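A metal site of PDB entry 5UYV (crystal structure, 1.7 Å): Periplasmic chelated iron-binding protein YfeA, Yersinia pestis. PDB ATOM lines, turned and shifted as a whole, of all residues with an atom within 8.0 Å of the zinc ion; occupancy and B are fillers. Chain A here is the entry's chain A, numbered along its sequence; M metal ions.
The side-chain carboxylate (OE2) of Glu 207 lies within hydrogen-bond range of the backbone NH (N) of Asn 228, 2.9 Å away. The side-chain amide oxygen (OD1) of Asn 139 is in hydrogen-bond range of a ring nitrogen (ND1) of His 141 (2.9 Å). The side-chain amide nitrogen (ND2) of Asn 228 sits at hydrogen-bond distance from the side-chain carboxylate (OE2) of Glu 74. N of His 76 is in hydrogen-bond range of OE2 of Glu 74. The side-chain amide oxygen of Asn 228 lies within hydrogen-bond range of the indole nitrogen of Trp 225 (2.8 Å). The backbone NH (N) of Glu 207 sits at hydrogen-bond distance from the side-chain carboxylate (OE1) of Glu 256, at 2.8 Å.
The zinc ion is bound by NE2 of His 76, NE2 of His 141, OE1 of Glu 207 and OD2 of Asp 282. Slightly farther from the zinc ion lies OE2 of Glu 207 (2.7 Å). Slightly farther from the zinc ion lies OD1 of Asp 282 (2.7 Å).
Asn 228 touches the zinc ion. Five residues have an atom within 4 Å of the zinc ion: His 76, His 141, Glu 207, Asn 228 and Asp 282. Along chain A the residues within 4 Å of the zinc ion span positions 76 to 282.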
ATOM      1  N   PHE A  48       1.093  18.314  -9.899  1.00  0.00           N
ATOM      2  CA  PHE A  48       1.237  18.194  -8.446  1.00  0.00           C
ATOM      3  C   PHE A  48       0.185  19.061  -7.771  1.00  0.00           C
ATOM      4  O   PHE A  48      -0.632  19.731  -8.425  1.00  0.00           O
ATOM      5  CB  PHE A  48       2.694  18.490  -7.995  1.00  0.00           C
ATOM      6  CG  PHE A  48       3.106  19.957  -7.972  1.00  0.00           C
ATOM      7  CD1 PHE A  48       3.274  20.662  -9.147  1.00  0.00           C
ATOM      8  CD2 PHE A  48       3.411  20.595  -6.759  1.00  0.00           C
ATOM      9  CE1 PHE A  48       3.689  21.996  -9.140  1.00  0.00           C
ATOM     10  CE2 PHE A  48       3.844  21.942  -6.746  1.00  0.00           C
ATOM     11  CZ  PHE A  48       3.967  22.628  -7.937  1.00  0.00           C
ATOM     12  N   GLU A  74       7.021  12.778  -3.284  1.00  0.00           N
ATOM     13  CA  GLU A  74       8.129  13.545  -3.824  1.00  0.00           C
ATOM     14  C   GLU A  74       7.895  13.835  -5.320  1.00  0.00           C
ATOM     15  O   GLU A  74       7.746  12.905  -6.117  1.00  0.00           O
ATOM     16  CB  GLU A  74       9.428  12.784  -3.579  1.00  0.00           C
ATOM     17  CG  GLU A  74      10.691  13.637  -3.565  1.00  0.00           C
ATOM     18  CD  GLU A  74      10.956  14.291  -4.896  1.00  0.00           C
ATOM     19  OE1 GLU A  74      11.255  13.553  -5.862  1.00  0.00           O
ATOM     20  OE2 GLU A  74      10.856  15.531  -4.986  1.00  0.00           O
ATOM     21  N   ILE A  75       7.872  15.115  -5.700  1.00  0.00           N
ATOM     22  CA  ILE A  75       7.404  15.486  -7.034  1.00  0.00           C
ATOM     23  C   ILE A  75       8.514  15.661  -8.073  1.00  0.00           C
ATOM     24  O   ILE A  75       8.218  15.604  -9.274  1.00  0.00           O
ATOM     25  CB  ILE A  75       6.598  16.792  -6.995  1.00  0.00           C
ATOM     26  CG1 ILE A  75       7.491  17.973  -6.605  1.00  0.00           C
ATOM     27  CG2 ILE A  75       5.465  16.676  -5.972  1.00  0.00           C
ATOM     28  CD1 ILE A  75       6.712  19.309  -6.519  1.00  0.00           C
ATOM     29  N   HIS A  76       9.765  15.915  -7.659  1.00  0.00           N
ATOM     30  CA  HIS A  76      10.817  16.192  -8.630  1.00  0.00           C
ATOM     31  C   HIS A  76      11.164  14.953  -9.429  1.00  0.00           C
ATOM     32  O   HIS A  76      11.259  14.998 -10.663  1.00  0.00           O
ATOM     33  CB  HIS A  76      12.088  16.689  -7.937  1.00  0.00           C
ATOM     34  CG  HIS A  76      11.932  17.985  -7.191  1.00  0.00           C
ATOM     35  ND1 HIS A  76      12.457  19.177  -7.659  1.00  0.00           N
ATOM     36  CD2 HIS A  76      11.352  18.267  -6.001  1.00  0.00           C
ATOM     37  CE1 HIS A  76      12.176  20.137  -6.786  1.00  0.00           C
ATOM     38  NE2 HIS A  76      11.513  19.607  -5.777  1.00  0.00           N
ATOM     39  N   LEU A 101      11.040  21.556 -12.788  1.00  0.00           N
ATOM     40  CA  LEU A 101      10.472  20.902 -11.614  1.00  0.00           C
ATOM     41  C   LEU A 101      10.250  19.417 -11.860  1.00  0.00           C
ATOM     42  O   LEU A 101      10.847  18.547 -11.210  1.00  0.00           O
ATOM     43  CB  LEU A 101       9.143  21.559 -11.203  1.00  0.00           C
ATOM     44  CG  LEU A 101       8.508  20.886  -9.969  1.00  0.00           C
ATOM     45  CD1 LEU A 101       9.339  21.072  -8.676  1.00  0.00           C
ATOM     46  CD2 LEU A 101       7.083  21.357  -9.744  1.00  0.00           C
ATOM     47  N   ASN A 139      15.553  27.648 -10.460  1.00  0.00           N
ATOM     48  CA  ASN A 139      14.931  27.053  -9.300  1.00  0.00           C
ATOM     49  C   ASN A 139      13.424  26.954  -9.569  1.00  0.00           C
ATOM     50  O   ASN A 139      12.787  27.963  -9.871  1.00  0.00           O
ATOM     51  CB  ASN A 139      15.266  27.900  -8.045  1.00  0.00           C
ATOM     52  CG  ASN A 139      14.739  27.298  -6.751  1.00  0.00           C
ATOM     53  OD1 ASN A 139      13.660  26.720  -6.716  1.00  0.00           O
ATOM     54  ND2 ASN A 139      15.498  27.491  -5.666  1.00  0.00           N
ATOM     55  N   PRO A 140      12.817  25.758  -9.481  1.00  0.00           N
ATOM     56  CA  PRO A 140      11.400  25.640  -9.865  1.00  0.00           C
ATOM     57  C   PRO A 140      10.403  26.152  -8.836  1.00  0.00           C
ATOM     58  O   PRO A 140       9.236  26.353  -9.195  1.00  0.00           O
ATOM     59  CB  PRO A 140      11.225  24.127 -10.058  1.00  0.00           C
ATOM     60  CG  PRO A 140      12.210  23.542  -9.052  1.00  0.00           C
ATOM     61  CD  PRO A 140      13.411  24.463  -9.147  1.00  0.00           C
ATOM     62  N   HIS A 141      10.808  26.373  -7.588  1.00  0.00           N
ATOM     63  CA  HIS A 141       9.823  26.582  -6.507  1.00  0.00           C
ATOM     64  C   HIS A 141       9.277  28.010  -6.466  1.00  0.00           C
ATOM     65  O   HIS A 141       9.173  28.613  -5.389  1.00  0.00           O
ATOM     66  CB  HIS A 141      10.433  26.226  -5.144  1.00  0.00           C
ATOM     67  CG  HIS A 141      10.988  24.828  -5.055  1.00  0.00           C
ATOM     68  ND1 HIS A 141      12.315  24.540  -5.307  1.00  0.00           N
ATOM     69  CD2 HIS A 141      10.401  23.651  -4.734  1.00  0.00           C
ATOM     70  CE1 HIS A 141      12.525  23.247  -5.138  1.00  0.00           C
ATOM     71  NE2 HIS A 141      11.385  22.677  -4.792  1.00  0.00           N
ATOM     72  N   TRP A 143       6.335  29.263  -6.730  1.00  0.00           N
ATOM     73  CA  TRP A 143       5.051  29.475  -6.068  1.00  0.00           C
ATOM     74  C   TRP A 143       5.181  29.888  -4.608  1.00  0.00           C
ATOM     75  O   TRP A 143       4.185  30.291  -4.004  1.00  0.00           O
ATOM     76  CB  TRP A 143       4.189  28.215  -6.152  1.00  0.00           C
ATOM     77  CG  TRP A 143       4.780  27.028  -5.456  1.00  0.00           C
ATOM     78  CD1 TRP A 143       4.670  26.705  -4.124  1.00  0.00           C
ATOM     79  CD2 TRP A 143       5.584  26.010  -6.054  1.00  0.00           C
ATOM     80  NE1 TRP A 143       5.358  25.523  -3.872  1.00  0.00           N
ATOM     81  CE2 TRP A 143       5.944  25.102  -5.035  1.00  0.00           C
ATOM     82  CE3 TRP A 143       6.057  25.805  -7.365  1.00  0.00           C
ATOM     83  CZ2 TRP A 143       6.739  23.966  -5.293  1.00  0.00           C
ATOM     84  CZ3 TRP A 143       6.853  24.683  -7.621  1.00  0.00           C
ATOM     85  CH2 TRP A 143       7.181  23.782  -6.589  1.00  0.00           C
ATOM     86  N   GLU A 207      15.877  20.830   1.603  1.00  0.00           N
ATOM     87  CA  GLU A 207      15.941  21.274   0.205  1.00  0.00           C
ATOM     88  C   GLU A 207      16.002  22.797   0.163  1.00  0.00           C
ATOM     89  O   GLU A 207      15.324  23.484   0.935  1.00  0.00           O
ATOM     90  CB  GLU A 207      14.730  20.787  -0.600  1.00  0.00           C
ATOM     91  CG  GLU A 207      14.885  21.070  -2.119  1.00  0.00           C
ATOM     92  CD  GLU A 207      13.671  20.741  -3.015  1.00  0.00           C
ATOM     93  OE1 GLU A 207      12.497  20.713  -2.544  1.00  0.00           O
ATOM     94  OE2 GLU A 207      13.903  20.575  -4.242  1.00  0.00           O
ATOM     95  N   GLY A 208      16.769  23.333  -0.781  1.00  0.00           N
ATOM     96  CA  GLY A 208      16.821  24.768  -1.013  1.00  0.00           C
ATOM     97  C   GLY A 208      15.594  25.229  -1.777  1.00  0.00           C
ATOM     98  O   GLY A 208      15.693  25.900  -2.807  1.00  0.00           O
ATOM     99  N   ALA A 209      14.421  24.883  -1.242  1.00  0.00           N
ATOM    100  CA  ALA A 209      13.166  25.077  -1.957  1.00  0.00           C
ATOM    101  C   ALA A 209      12.541  26.430  -1.705  1.00  0.00           C
ATOM    102  O   ALA A 209      11.451  26.703  -2.242  1.00  0.00           O
ATOM    103  CB  ALA A 209      12.158  23.994  -1.558  1.00  0.00           C
ATOM    104  N   PHE A 210      13.185  27.286  -0.918  1.00  0.00           N
ATOM    105  CA  PHE A 210      12.535  28.496  -0.419  1.00  0.00           C
ATOM    106  C   PHE A 210      13.160  29.765  -0.976  1.00  0.00           C
ATOM    107  O   PHE A 210      12.890  30.850  -0.455  1.00  0.00           O
ATOM    108  CB  PHE A 210      12.549  28.478   1.110  1.00  0.00           C
ATOM    109  CG  PHE A 210      11.820  27.309   1.678  1.00  0.00           C
ATOM    110  CD1 PHE A 210      10.443  27.362   1.872  1.00  0.00           C
ATOM    111  CD2 PHE A 210      12.483  26.115   1.906  1.00  0.00           C
ATOM    112  CE1 PHE A 210       9.747  26.265   2.357  1.00  0.00           C
ATOM    113  CE2 PHE A 210      11.802  24.998   2.371  1.00  0.00           C
ATOM    114  CZ  PHE A 210      10.421  25.078   2.592  1.00  0.00           C
ATOM    115  N   TRP A 225      20.571  20.503   0.711  1.00  0.00           N
ATOM    116  CA  TRP A 225      20.834  20.176  -0.687  1.00  0.00           C
ATOM    117  C   TRP A 225      20.101  21.158  -1.584  1.00  0.00           C
ATOM    118  O   TRP A 225      19.003  21.596  -1.239  1.00  0.00           O
ATOM    119  CB  TRP A 225      20.450  18.741  -1.045  1.00  0.00           C
ATOM    120  CG  TRP A 225      19.028  18.319  -0.707  1.00  0.00           C
ATOM    121  CD1 TRP A 225      17.923  18.405  -1.508  1.00  0.00           C
ATOM    122  CD2 TRP A 225      18.580  17.708   0.519  1.00  0.00           C
ATOM    123  NE1 TRP A 225      16.814  17.891  -0.865  1.00  0.00           N
ATOM    124  CE2 TRP A 225      17.196  17.465   0.391  1.00  0.00           C
ATOM    125  CE3 TRP A 225      19.223  17.354   1.705  1.00  0.00           C
ATOM    126  CZ2 TRP A 225      16.432  16.874   1.393  1.00  0.00           C
ATOM    127  CZ3 TRP A 225      18.469  16.769   2.714  1.00  0.00           C
ATOM    128  CH2 TRP A 225      17.093  16.536   2.551  1.00  0.00           C
ATOM    129  N   PRO A 226      20.691  21.552  -2.719  1.00  0.00           N
ATOM    130  CA  PRO A 226      20.112  22.667  -3.481  1.00  0.00           C
ATOM    131  C   PRO A 226      18.761  22.336  -4.102  1.00  0.00           C
ATOM    132  O   PRO A 226      17.885  23.214  -4.175  1.00  0.00           O
ATOM    133  CB  PRO A 226      21.182  22.967  -4.556  1.00  0.00           C
ATOM    134  CG  PRO A 226      22.081  21.777  -4.568  1.00  0.00           C
ATOM    135  CD  PRO A 226      22.036  21.166  -3.206  1.00  0.00           C
ATOM    136  N   ILE A 227      18.574  21.105  -4.565  1.00  0.00           N
ATOM    137  CA  ILE A 227      17.298  20.675  -5.140  1.00  0.00           C
ATOM    138  C   ILE A 227      17.220  19.156  -4.993  1.00  0.00           C
ATOM    139  O   ILE A 227      18.231  18.451  -5.046  1.00  0.00           O
ATOM    140  CB  ILE A 227      17.160  21.131  -6.616  1.00  0.00           C
ATOM    141  CG1 ILE A 227      15.782  20.782  -7.193  1.00  0.00           C
ATOM    142  CG2 ILE A 227      18.281  20.531  -7.500  1.00  0.00           C
ATOM    143  CD1 ILE A 227      15.450  21.504  -8.516  1.00  0.00           C
ATOM    144  N   ASN A 228      16.007  18.677  -4.760  1.00  0.00           N
ATOM    145  CA  ASN A 228      15.797  17.239  -4.614  1.00  0.00           C
ATOM    146  C   ASN A 228      16.403  16.501  -5.797  1.00  0.00           C
ATOM    147  O   ASN A 228      16.193  16.878  -6.956  1.00  0.00           O
ATOM    148  CB  ASN A 228      14.295  16.934  -4.514  1.00  0.00           C
ATOM    149  CG  ASN A 228      13.710  17.388  -3.184  1.00  0.00           C
ATOM    150  OD1 ASN A 228      14.407  17.910  -2.322  1.00  0.00           O
ATOM    151  ND2 ASN A 228      12.398  17.165  -3.013  1.00  0.00           N
ATOM    152  N   GLU A 256      11.147  19.512   5.293  1.00  0.00           N
ATOM    153  CA  GLU A 256       9.991  19.753   4.432  1.00  0.00           C
ATOM    154  C   GLU A 256       9.167  18.478   4.276  1.00  0.00           C
ATOM    155  O   GLU A 256       9.651  17.367   4.502  1.00  0.00           O
ATOM    156  CB  GLU A 256      10.421  20.267   3.050  1.00  0.00           C
ATOM    157  CG  GLU A 256      11.221  21.546   3.097  1.00  0.00           C
ATOM    158  CD  GLU A 256      12.710  21.269   3.214  1.00  0.00           C
ATOM    159  OE1 GLU A 256      13.218  20.517   2.343  1.00  0.00           O
ATOM    160  OE2 GLU A 256      13.346  21.790   4.167  1.00  0.00           O
ATOM    161  N   THR A 258       7.830  16.462   2.025  1.00  0.00           N
ATOM    162  CA  THR A 258       7.974  15.306   1.146  1.00  0.00           C
ATOM    163  C   THR A 258       9.325  14.622   1.246  1.00  0.00           C
ATOM    164  O   THR A 258       9.560  13.657   0.501  1.00  0.00           O
ATOM    165  CB  THR A 258       7.738  15.658  -0.332  1.00  0.00           C
ATOM    166  OG1 THR A 258       8.828  16.462  -0.806  1.00  0.00           O
ATOM    167  CG2 THR A 258       6.396  16.393  -0.518  1.00  0.00           C
ATOM    168  N   ILE A 259      10.219  15.088   2.117  1.00  0.00           N
ATOM    169  CA  ILE A 259      11.557  14.522   2.245  1.00  0.00           C
ATOM    170  C   ILE A 259      11.795  14.150   3.709  1.00  0.00           C
ATOM    171  O   ILE A 259      10.952  14.376   4.579  1.00  0.00           O
ATOM    172  CB  ILE A 259      12.645  15.475   1.700  1.00  0.00           C
ATOM    173  CG1 ILE A 259      12.477  16.899   2.225  1.00  0.00           C
ATOM    174  CG2 ILE A 259      12.599  15.499   0.185  1.00  0.00           C
ATOM    175  CD1 ILE A 259      13.066  17.148   3.583  1.00  0.00           C
ATOM    176  N   VAL A 281       6.106  22.851   1.040  1.00  0.00           N
ATOM    177  CA  VAL A 281       6.500  23.575  -0.163  1.00  0.00           C
ATOM    178  C   VAL A 281       6.137  22.748  -1.393  1.00  0.00           C
ATOM    179  O   VAL A 281       5.522  23.262  -2.323  1.00  0.00           O
ATOM    180  CB  VAL A 281       7.996  23.956  -0.165  1.00  0.00           C
ATOM    181  CG1 VAL A 281       8.927  22.775   0.246  1.00  0.00           C
ATOM    182  CG2 VAL A 281       8.395  24.507  -1.563  1.00  0.00           C
ATOM    183  N   ASP A 282       6.492  21.469  -1.393  1.00  0.00           N
ATOM    184  CA  ASP A 282       6.317  20.679  -2.611  1.00  0.00           C
ATOM    185  C   ASP A 282       4.976  19.953  -2.677  1.00  0.00           C
ATOM    186  O   ASP A 282       4.641  19.401  -3.738  1.00  0.00           O
ATOM    187  CB  ASP A 282       7.453  19.657  -2.728  1.00  0.00           C
ATOM    188  CG  ASP A 282       8.728  20.261  -3.301  1.00  0.00           C
ATOM    189  OD1 ASP A 282       8.705  21.436  -3.704  1.00  0.00           O
ATOM    190  OD2 ASP A 282       9.736  19.547  -3.343  1.00  0.00           O
ATOM    191  N   SER A 283       4.216  19.929  -1.585  1.00  0.00           N
ATOM    192  CA  SER A 283       2.934  19.267  -1.582  1.00  0.00           C
ATOM    193  C   SER A 283       2.020  19.889  -0.532  1.00  0.00           C
ATOM    194  O   SER A 283       2.486  20.342   0.507  1.00  0.00           O
ATOM    195  CB  SER A 283       3.077  17.760  -1.308  1.00  0.00           C
ATOM    196  OG  SER A 283       1.813  17.128  -1.332  1.00  0.00           O
HETATM  197 ZN    ZN M   1      11.242  20.744  -4.159  1.00  0.00          ZN
